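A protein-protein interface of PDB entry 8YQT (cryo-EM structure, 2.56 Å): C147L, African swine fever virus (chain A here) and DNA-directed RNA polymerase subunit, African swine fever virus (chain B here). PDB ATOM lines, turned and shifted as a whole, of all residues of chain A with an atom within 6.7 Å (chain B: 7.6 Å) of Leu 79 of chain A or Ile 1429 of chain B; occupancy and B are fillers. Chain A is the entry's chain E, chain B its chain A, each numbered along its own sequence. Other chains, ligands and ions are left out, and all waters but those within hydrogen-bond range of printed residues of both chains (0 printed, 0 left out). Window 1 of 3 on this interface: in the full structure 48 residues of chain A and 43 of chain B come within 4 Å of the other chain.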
ATOM      1  N   LEU A  71     -18.450  -0.413  17.636  1.00  0.00           N
ATOM      2  CA  LEU A  71     -17.212  -0.844  18.261  1.00  0.00           C
ATOM      3  C   LEU A  71     -17.120  -0.312  19.683  1.00  0.00           C
ATOM      4  O   LEU A  71     -17.493   0.828  19.969  1.00  0.00           O
ATOM      5  CB  LEU A  71     -16.009  -0.355  17.458  1.00  0.00           C
ATOM      6  CG  LEU A  71     -15.685  -1.060  16.150  1.00  0.00           C
ATOM      7  CD1 LEU A  71     -14.760  -0.196  15.324  1.00  0.00           C
ATOM      8  CD2 LEU A  71     -15.052  -2.405  16.432  1.00  0.00           C
ATOM      9  N   PHE A  74     -12.494  -0.351  23.739  1.00  0.00           N
ATOM     10  CA  PHE A  74     -11.447  -1.367  23.766  1.00  0.00           C
ATOM     11  C   PHE A  74     -11.155  -1.897  22.368  1.00  0.00           C
ATOM     12  O   PHE A  74      -9.994  -2.009  21.964  1.00  0.00           O
ATOM     13  CB  PHE A  74     -11.867  -2.511  24.685  1.00  0.00           C
ATOM     14  CG  PHE A  74     -11.921  -2.145  26.132  1.00  0.00           C
ATOM     15  CD1 PHE A  74     -11.044  -1.222  26.659  1.00  0.00           C
ATOM     16  CD2 PHE A  74     -12.852  -2.732  26.970  1.00  0.00           C
ATOM     17  CE1 PHE A  74     -11.092  -0.893  27.991  1.00  0.00           C
ATOM     18  CE2 PHE A  74     -12.902  -2.404  28.300  1.00  0.00           C
ATOM     19  CZ  PHE A  74     -12.021  -1.483  28.811  1.00  0.00           C
ATOM     20  N   GLU A  75     -12.206  -2.229  21.614  1.00  0.00           N
ATOM     21  CA  GLU A  75     -12.021  -2.790  20.281  1.00  0.00           C
ATOM     22  C   GLU A  75     -11.407  -1.779  19.323  1.00  0.00           C
ATOM     23  O   GLU A  75     -10.527  -2.128  18.533  1.00  0.00           O
ATOM     24  CB  GLU A  75     -13.353  -3.302  19.737  1.00  0.00           C
ATOM     25  CG  GLU A  75     -13.757  -4.650  20.286  1.00  0.00           C
ATOM     26  CD  GLU A  75     -15.210  -4.981  20.025  1.00  0.00           C
ATOM     27  OE1 GLU A  75     -15.950  -4.097  19.552  1.00  0.00           O
ATOM     28  OE2 GLU A  75     -15.615  -6.128  20.304  1.00  0.00           O
ATOM     29  N   ALA A  76     -11.866  -0.526  19.362  1.00  0.00           N
ATOM     30  CA  ALA A  76     -11.292   0.495  18.493  1.00  0.00           C
ATOM     31  C   ALA A  76      -9.834   0.766  18.842  1.00  0.00           C
ATOM     32  O   ALA A  76      -8.994   0.922  17.949  1.00  0.00           O
ATOM     33  CB  ALA A  76     -12.114   1.776  18.573  1.00  0.00           C
ATOM     34  N   THR A  77      -9.515   0.824  20.136  1.00  0.00           N
ATOM     35  CA  THR A  77      -8.127   1.001  20.546  1.00  0.00           C
ATOM     36  C   THR A  77      -7.263  -0.160  20.076  1.00  0.00           C
ATOM     37  O   THR A  77      -6.149   0.047  19.581  1.00  0.00           O
ATOM     38  CB  THR A  77      -8.045   1.149  22.065  1.00  0.00           C
ATOM     39  OG1 THR A  77      -8.876   2.236  22.485  1.00  0.00           O
ATOM     40  CG2 THR A  77      -6.621   1.416  22.503  1.00  0.00           C
ATOM     41  N   ARG A  78      -7.760  -1.389  20.218  1.00  0.00           N
ATOM     42  CA  ARG A  78      -7.017  -2.559  19.763  1.00  0.00           C
ATOM     43  C   ARG A  78      -6.818  -2.539  18.253  1.00  0.00           C
ATOM     44  O   ARG A  78      -5.730  -2.854  17.762  1.00  0.00           O
ATOM     45  CB  ARG A  78      -7.745  -3.829  20.197  1.00  0.00           C
ATOM     46  CG  ARG A  78      -7.131  -5.121  19.701  1.00  0.00           C
ATOM     47  CD  ARG A  78      -5.751  -5.363  20.278  1.00  0.00           C
ATOM     48  NE  ARG A  78      -5.271  -6.697  19.940  1.00  0.00           N
ATOM     49  CZ  ARG A  78      -4.013  -7.096  20.054  1.00  0.00           C
ATOM     50  NH1 ARG A  78      -3.068  -6.285  20.495  1.00  0.00           N
ATOM     51  NH2 ARG A  78      -3.696  -8.341  19.714  1.00  0.00           N
ATOM     52  N   LEU A  79      -7.855  -2.166  17.502  1.00  0.00           N
ATOM     53  CA  LEU A  79      -7.741  -2.089  16.051  1.00  0.00           C
ATOM     54  C   LEU A  79      -6.690  -1.071  15.639  1.00  0.00           C
ATOM     55  O   LEU A  79      -5.843  -1.347  14.782  1.00  0.00           O
ATOM     56  CB  LEU A  79      -9.094  -1.730  15.437  1.00  0.00           C
ATOM     57  CG  LEU A  79     -10.147  -2.827  15.335  1.00  0.00           C
ATOM     58  CD1 LEU A  79     -11.505  -2.212  15.088  1.00  0.00           C
ATOM     59  CD2 LEU A  79      -9.792  -3.792  14.230  1.00  0.00           C
ATOM     60  N   VAL A  80      -6.725   0.114  16.251  1.00  0.00           N
ATOM     61  CA  VAL A  80      -5.771   1.156  15.892  1.00  0.00           C
ATOM     62  C   VAL A  80      -4.355   0.747  16.277  1.00  0.00           C
ATOM     63  O   VAL A  80      -3.411   0.968  15.516  1.00  0.00           O
ATOM     64  CB  VAL A  80      -6.179   2.497  16.528  1.00  0.00           C
ATOM     65  CG1 VAL A  80      -5.100   3.535  16.326  1.00  0.00           C
ATOM     66  CG2 VAL A  80      -7.474   2.985  15.928  1.00  0.00           C
ATOM     67  N   ALA A  81      -4.182   0.132  17.449  1.00  0.00           N
ATOM     68  CA  ALA A  81      -2.848  -0.285  17.871  1.00  0.00           C
ATOM     69  C   ALA A  81      -2.288  -1.362  16.951  1.00  0.00           C
ATOM     70  O   ALA A  81      -1.127  -1.291  16.524  1.00  0.00           O
ATOM     71  CB  ALA A  81      -2.886  -0.781  19.315  1.00  0.00           C
ATOM     72  N   VAL A  82      -3.107  -2.363  16.623  1.00  0.00           N
ATOM     73  CA  VAL A  82      -2.660  -3.432  15.739  1.00  0.00           C
ATOM     74  C   VAL A  82      -2.293  -2.869  14.376  1.00  0.00           C
ATOM     75  O   VAL A  82      -1.218  -3.156  13.842  1.00  0.00           O
ATOM     76  CB  VAL A  82      -3.739  -4.525  15.627  1.00  0.00           C
ATOM     77  CG1 VAL A  82      -3.466  -5.422  14.434  1.00  0.00           C
ATOM     78  CG2 VAL A  82      -3.796  -5.343  16.900  1.00  0.00           C
ATOM     79  N   ARG A  83      -3.165  -2.032  13.808  1.00  0.00           N
ATOM     80  CA  ARG A  83      -2.910  -1.480  12.484  1.00  0.00           C
ATOM     81  C   ARG A  83      -1.691  -0.569  12.473  1.00  0.00           C
ATOM     82  O   ARG A  83      -0.932  -0.566  11.499  1.00  0.00           O
ATOM     83  CB  ARG A  83      -4.142  -0.730  11.987  1.00  0.00           C
ATOM     84  CG  ARG A  83      -3.986  -0.158  10.598  1.00  0.00           C
ATOM     85  CD  ARG A  83      -3.630  -1.249   9.609  1.00  0.00           C
ATOM     86  NE  ARG A  83      -3.348  -0.709   8.287  1.00  0.00           N
ATOM     87  CZ  ARG A  83      -2.775  -1.394   7.308  1.00  0.00           C
ATOM     88  NH1 ARG A  83      -2.416  -2.655   7.468  1.00  0.00           N
ATOM     89  NH2 ARG A  83      -2.558  -0.798   6.140  1.00  0.00           N
ATOM     90  N   ALA A  84      -1.486   0.212  13.535  1.00  0.00           N
ATOM     91  CA  ALA A  84      -0.297   1.045  13.627  1.00  0.00           C
ATOM     92  C   ALA A  84       0.968   0.207  13.686  1.00  0.00           C
ATOM     93  O   ALA A  84       1.978   0.571  13.075  1.00  0.00           O
ATOM     94  CB  ALA A  84      -0.393   1.955  14.849  1.00  0.00           C
ATOM     95  N   ALA A 106      -3.278   5.062  11.278  1.00  0.00           N
ATOM     96  CA  ALA A 106      -4.224   4.065  11.770  1.00  0.00           C
ATOM     97  C   ALA A 106      -5.550   4.697  12.182  1.00  0.00           C
ATOM     98  O   ALA A 106      -6.621   4.180  11.841  1.00  0.00           O
ATOM     99  CB  ALA A 106      -3.608   3.296  12.935  1.00  0.00           C
ATOM    100  N   LEU A 110      -9.181   4.067  10.414  1.00  0.00           N
ATOM    101  CA  LEU A 110     -10.376   3.657  11.143  1.00  0.00           C
ATOM    102  C   LEU A 110     -11.522   4.634  10.918  1.00  0.00           C
ATOM    103  O   LEU A 110     -12.666   4.223  10.697  1.00  0.00           O
ATOM    104  CB  LEU A 110     -10.066   3.532  12.633  1.00  0.00           C
ATOM    105  CG  LEU A 110     -11.256   3.164  13.519  1.00  0.00           C
ATOM    106  CD1 LEU A 110     -11.622   1.703  13.343  1.00  0.00           C
ATOM    107  CD2 LEU A 110     -10.966   3.476  14.969  1.00  0.00           C
ATOM    108  N   ILE A 115      -9.824   0.373   7.146  1.00  0.00           N
ATOM    109  CA  ILE A 115      -8.922  -0.461   7.941  1.00  0.00           C
ATOM    110  C   ILE A 115      -9.085  -1.919   7.518  1.00  0.00           C
ATOM    111  O   ILE A 115     -10.220  -2.419   7.464  1.00  0.00           O
ATOM    112  CB  ILE A 115      -9.202  -0.268   9.433  1.00  0.00           C
ATOM    113  CG1 ILE A 115      -8.262  -1.111  10.291  1.00  0.00           C
ATOM    114  CG2 ILE A 115     -10.666  -0.531   9.766  1.00  0.00           C
ATOM    115  CD1 ILE A 115      -8.158  -0.615  11.708  1.00  0.00           C
ATOM    116  N   LEU A 117      -8.941  -4.874   8.759  1.00  0.00           N
ATOM    117  CA  LEU A 117      -9.012  -5.780   9.891  1.00  0.00           C
ATOM    118  C   LEU A 117     -10.459  -6.182  10.129  1.00  0.00           C
ATOM    119  O   LEU A 117     -11.390  -5.492   9.715  1.00  0.00           O
ATOM    120  CB  LEU A 117      -8.424  -5.144  11.155  1.00  0.00           C
ATOM    121  CG  LEU A 117      -6.932  -4.815  11.118  1.00  0.00           C
ATOM    122  CD1 LEU A 117      -6.503  -4.095  12.377  1.00  0.00           C
ATOM    123  CD2 LEU A 117      -6.130  -6.076  10.936  1.00  0.00           C
ATOM    124  N   LEU A 118     -10.635  -7.321  10.788  1.00  0.00           N
ATOM    125  CA  LEU A 118     -11.947  -7.795  11.194  1.00  0.00           C
ATOM    126  C   LEU A 118     -11.924  -8.118  12.679  1.00  0.00           C
ATOM    127  O   LEU A 118     -10.910  -8.565  13.216  1.00  0.00           O
ATOM    128  CB  LEU A 118     -12.379  -9.033  10.403  1.00  0.00           C
ATOM    129  CG  LEU A 118     -12.635  -8.878   8.905  1.00  0.00           C
ATOM    130  CD1 LEU A 118     -12.878 -10.236   8.282  1.00  0.00           C
ATOM    131  CD2 LEU A 118     -13.810  -7.956   8.656  1.00  0.00           C
ATOM    132  N   VAL A 119     -13.053  -7.886  13.339  1.00  0.00           N
ATOM    133  CA  VAL A 119     -13.205  -8.165  14.760  1.00  0.00           C
ATOM    134  C   VAL A 119     -13.927  -9.492  14.914  1.00  0.00           C
ATOM    135  O   VAL A 119     -15.021  -9.678  14.369  1.00  0.00           O
ATOM    136  CB  VAL A 119     -13.973  -7.038  15.473  1.00  0.00           C
ATOM    137  CG1 VAL A 119     -14.062  -7.320  16.964  1.00  0.00           C
ATOM    138  CG2 VAL A 119     -13.314  -5.702  15.218  1.00  0.00           C
ATOM    139  N   MET A 120     -13.318 -10.417  15.646  1.00  0.00           N
ATOM    140  CA  MET A 120     -13.937 -11.697  15.956  1.00  0.00           C
ATOM    141  C   MET A 120     -14.336 -11.712  17.424  1.00  0.00           C
ATOM    142  O   MET A 120     -13.490 -11.536  18.305  1.00  0.00           O
ATOM    143  CB  MET A 120     -12.998 -12.859  15.644  1.00  0.00           C
ATOM    144  CG  MET A 120     -13.624 -14.222  15.877  1.00  0.00           C
ATOM    145  SD  MET A 120     -12.401 -15.525  16.076  1.00  0.00           S
ATOM    146  CE  MET A 120     -12.175 -16.002  14.368  1.00  0.00           C
ATOM    147  N   PRO A 138     -15.253  -3.639  10.893  1.00  0.00           N
ATOM    148  CA  PRO A 138     -15.194  -2.277  11.444  1.00  0.00           C
ATOM    149  C   PRO A 138     -15.432  -1.186  10.419  1.00  0.00           C
ATOM    150  O   PRO A 138     -15.734  -0.054  10.812  1.00  0.00           O
ATOM    151  CB  PRO A 138     -13.777  -2.194  12.026  1.00  0.00           C
ATOM    152  CG  PRO A 138     -13.018  -3.259  11.342  1.00  0.00           C
ATOM    153  CD  PRO A 138     -13.988  -4.361  11.084  1.00  0.00           C
ATOM    154  N   MET A 141     -19.149  -0.494  10.879  1.00  0.00           N
ATOM    155  CA  MET A 141     -19.540  -0.393  12.274  1.00  0.00           C
ATOM    156  C   MET A 141     -19.547   1.059  12.725  1.00  0.00           C
ATOM    157  O   MET A 141     -18.912   1.925  12.121  1.00  0.00           O
ATOM    158  CB  MET A 141     -18.588  -1.202  13.162  1.00  0.00           C
ATOM    159  CG  MET A 141     -18.891  -2.682  13.221  1.00  0.00           C
ATOM    160  SD  MET A 141     -17.736  -3.553  14.285  1.00  0.00           S
ATOM    161  CE  MET A 141     -18.835  -4.093  15.586  1.00  0.00           C
ATOM    162  N   VAL B 475      -0.624   3.989  21.502  1.00  0.00           N
ATOM    163  CA  VAL B 475      -2.008   4.104  21.049  1.00  0.00           C
ATOM    164  C   VAL B 475      -2.964   3.922  22.216  1.00  0.00           C
ATOM    165  O   VAL B 475      -3.931   4.675  22.376  1.00  0.00           O
ATOM    166  CB  VAL B 475      -2.290   3.084  19.932  1.00  0.00           C
ATOM    167  CG1 VAL B 475      -3.775   3.025  19.639  1.00  0.00           C
ATOM    168  CG2 VAL B 475      -1.510   3.429  18.687  1.00  0.00           C
ATOM    169  N   LEU B 479      -5.723   6.752  23.775  1.00  0.00           N
ATOM    170  CA  LEU B 479      -7.112   6.438  23.461  1.00  0.00           C
ATOM    171  C   LEU B 479      -7.881   5.891  24.651  1.00  0.00           C
ATOM    172  O   LEU B 479      -9.096   6.085  24.737  1.00  0.00           O
ATOM    173  CB  LEU B 479      -7.188   5.436  22.307  1.00  0.00           C
ATOM    174  CG  LEU B 479      -6.859   5.971  20.914  1.00  0.00           C
ATOM    175  CD1 LEU B 479      -7.115   4.911  19.857  1.00  0.00           C
ATOM    176  CD2 LEU B 479      -7.658   7.223  20.622  1.00  0.00           C
ATOM    177  N   THR B1424      -8.706  -4.486  25.986  1.00  0.00           N
ATOM    178  CA  THR B1424      -8.279  -4.479  24.594  1.00  0.00           C
ATOM    179  C   THR B1424      -7.961  -5.870  24.068  1.00  0.00           C
ATOM    180  O   THR B1424      -7.803  -6.030  22.855  1.00  0.00           O
ATOM    181  CB  THR B1424      -7.062  -3.572  24.414  1.00  0.00           C
ATOM    182  OG1 THR B1424      -6.090  -3.864  25.422  1.00  0.00           O
ATOM    183  CG2 THR B1424      -7.465  -2.119  24.511  1.00  0.00           C
ATOM    184  N   TYR B1426      -9.990  -8.575  24.892  1.00  0.00           N
ATOM    185  CA  TYR B1426     -11.189  -9.395  24.982  1.00  0.00           C
ATOM    186  C   TYR B1426     -11.614  -9.934  23.622  1.00  0.00           C
ATOM    187  O   TYR B1426     -12.056 -11.081  23.529  1.00  0.00           O
ATOM    188  CB  TYR B1426     -12.332  -8.603  25.614  1.00  0.00           C
ATOM    189  CG  TYR B1426     -13.457  -9.492  26.073  1.00  0.00           C
ATOM    190  CD1 TYR B1426     -13.272 -10.376  27.119  1.00  0.00           C
ATOM    191  CD2 TYR B1426     -14.696  -9.459  25.456  1.00  0.00           C
ATOM    192  CE1 TYR B1426     -14.281 -11.198  27.539  1.00  0.00           C
ATOM    193  CE2 TYR B1426     -15.715 -10.280  25.874  1.00  0.00           C
ATOM    194  CZ  TYR B1426     -15.498 -11.148  26.914  1.00  0.00           C
ATOM    195  OH  TYR B1426     -16.503 -11.977  27.341  1.00  0.00           O
ATOM    196  N   SER B1427     -11.485  -9.134  22.569  1.00  0.00           N
ATOM    197  CA  SER B1427     -11.883  -9.529  21.229  1.00  0.00           C
ATOM    198  C   SER B1427     -10.655  -9.860  20.392  1.00  0.00           C
ATOM    199  O   SER B1427      -9.588  -9.265  20.557  1.00  0.00           O
ATOM    200  CB  SER B1427     -12.689  -8.424  20.546  1.00  0.00           C
ATOM    201  OG  SER B1427     -13.894  -8.172  21.241  1.00  0.00           O
ATOM    202  N   ASP B1428     -10.819 -10.821  19.489  1.00  0.00           N
ATOM    203  CA  ASP B1428      -9.748 -11.222  18.592  1.00  0.00           C
ATOM    204  C   ASP B1428      -9.805 -10.414  17.305  1.00  0.00           C
ATOM    205  O   ASP B1428     -10.884 -10.130  16.780  1.00  0.00           O
ATOM    206  CB  ASP B1428      -9.840 -12.713  18.269  1.00  0.00           C
ATOM    207  CG  ASP B1428      -9.872 -13.575  19.510  1.00  0.00           C
ATOM    208  OD1 ASP B1428      -9.336 -13.147  20.553  1.00  0.00           O
ATOM    209  OD2 ASP B1428     -10.431 -14.689  19.441  1.00  0.00           O
ATOM    210  N   ILE B1429      -8.635 -10.040  16.806  1.00  0.00           N
ATOM    211  CA  ILE B1429      -8.507  -9.342  15.534  1.00  0.00           C
ATOM    212  C   ILE B1429      -7.967 -10.327  14.509  1.00  0.00           C
ATOM    213  O   ILE B1429      -6.974 -11.017  14.765  1.00  0.00           O
ATOM    214  CB  ILE B1429      -7.589  -8.115  15.657  1.00  0.00           C
ATOM    215  CG1 ILE B1429      -7.985  -7.263  16.862  1.00  0.00           C
ATOM    216  CG2 ILE B1429      -7.648  -7.290  14.391  1.00  0.00           C
ATOM    217  CD1 ILE B1429      -9.378  -6.705  16.786  1.00  0.00           C
ATOM    218  N   ILE B1430      -8.627 -10.406  13.358  1.00  0.00           N
ATOM    219  CA  ILE B1430      -8.164 -11.242  12.262  1.00  0.00           C
ATOM    220  C   ILE B1430      -7.966 -10.360  11.040  1.00  0.00           C
ATOM    221  O   ILE B1430      -8.571  -9.296  10.902  1.00  0.00           O
ATOM    222  CB  ILE B1430      -9.129 -12.405  11.952  1.00  0.00           C
ATOM    223  CG1 ILE B1430     -10.449 -11.881  11.398  1.00  0.00           C
ATOM    224  CG2 ILE B1430      -9.373 -13.235  13.188  1.00  0.00           C
ATOM    225  CD1 ILE B1430     -11.414 -12.966  11.009  1.00  0.00           C
ATOM    226  N   MET B1431      -7.090 -10.812  10.152  1.00  0.00           N
ATOM    227  CA  MET B1431      -6.797 -10.070   8.938  1.00  0.00           C
ATOM    228  C   MET B1431      -7.971 -10.183   7.975  1.00  0.00           C
ATOM    229  O   MET B1431      -8.587 -11.245   7.850  1.00  0.00           O
ATOM    230  CB  MET B1431      -5.528 -10.611   8.285  1.00  0.00           C
ATOM    231  CG  MET B1431      -4.234 -10.208   8.974  1.00  0.00           C
ATOM    232  SD  MET B1431      -4.121  -8.482   9.455  1.00  0.00           S
ATOM    233  CE  MET B1431      -3.549  -7.738   7.940  1.00  0.00           C
ATOM    234  N   ASP B1432      -8.284  -9.084   7.295  1.00  0.00           N
ATOM    235  CA  ASP B1432      -9.376  -9.063   6.324  1.00  0.00           C
ATOM    236  C   ASP B1432      -8.812  -9.468   4.967  1.00  0.00           C
ATOM    237  O   ASP B1432      -8.342  -8.625   4.201  1.00  0.00           O
ATOM    238  CB  ASP B1432     -10.031  -7.688   6.274  1.00  0.00           C
ATOM    239  CG  ASP B1432     -11.397  -7.720   5.626  1.00  0.00           C
ATOM    240  OD1 ASP B1432     -11.794  -8.791   5.121  1.00  0.00           O
ATOM    241  OD2 ASP B1432     -12.080  -6.676   5.622  1.00  0.00           O
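O of Ile 1430 of chain B is in hydrogen-bond range of N of Leu 118 of chain A, at 2.9 Å. The backbone carbonyl oxygen of Asp 1428 of chain B lies within hydrogen-bond range of the backbone NH of Met 120 of chain A. The side-chain hydroxyl of Ser 1427 of chain B lies within hydrogen-bond range of the side-chain carboxylate of Glu 75 of chain A, 2.8 Å away.
Among the printed residues, pairs that only touch across the chains: Phe 74 of chain A with Thr 1424 of chain B, Thr 77 of chain A with Val 475 of chain B, Thr 77 of chain A with Leu 479 of chain B, Arg 78 of chain A with Thr 1424 of chain B, Arg 78 of chain A with Ile 1429 of chain B, Leu 79 of chain A with Ile 1429 of chain B, Val 80 of chain A with Val 475 of chain B, Ala 81 of chain A with Val 475 of chain B, Leu 117 of chain A with Ile 1429 of chain B, Leu 117 of chain A with Ile 1430 of chain B, Leu 117 of chain A with Met 1431 of chain B, Leu 117 of chain A with Asp 1432 of chain B, Leu 118 of chain A with Asp 1428 of chain B, Leu 118 of chain A with Ile 1429 of chain B, Leu 118 of chain A with Asp 1432 of chain B, Val 119 of chain A with Ser 1427 of chain B, Val 119 of chain A with Asp 1428 of chain B and Met 120 of chain A with Ser 1427 of chain B.
Printed residues of chain B within 4 Å of Arg 78 of chain A: Thr 1424 (3.4 Å) and Ile 1429 (3.7 Å). Leu 79 of chain A touches just one residue of chain B: Ile 1429 (3.9 Å). Printed residues of chain B within 4 Å of Ala 81 of chain A: Val 475 (3.7 Å). Arg 83 of chain A touches none of the printed residues of chain B. Met 141 of chain A touches none of the printed residues of chain B. Ile 1429 of chain B touches four residues of chain A. The nearest residue of chain B that does not touch Leu 79 of chain A is Val 475 of chain B (6.4 Å). The nearest printed residue of chain B that does not touch Met 120 of chain A is Ile 1430 of chain B (4.1 Å).
Of the 21 printed residues of chain A, 11 touch a printed residue of chain B. Hydrophobic or aromatic side chains of chain A within 4 Å of the printed part of chain B: Phe 74, Leu 79, Val 80, Ala 81, Leu 117, Leu 118, Val 119 and Met 120. Of the 10 printed residues of chain B, 9 touch a printed residue of chain A. Printed residues of chain B that touch a printed residue of chain A: Val 475, Leu 479, Thr 1424, Ser 1427, Asp 1428, Ile 1429, Ile 1430, Met 1431 and Asp 1432. Hydrophobic or aromatic side chains of chain B within 4 Å of the printed part of chain A: Val 475, Leu 479, Ile 1429, Ile 1430 and Met 1431. Among the printed residues, 21 pairs touch across the chains. Among the printed residues, no Asp or Glu carboxylate lies within 4 Å of a Lys or Arg side-chain nitrogen of the other chain.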
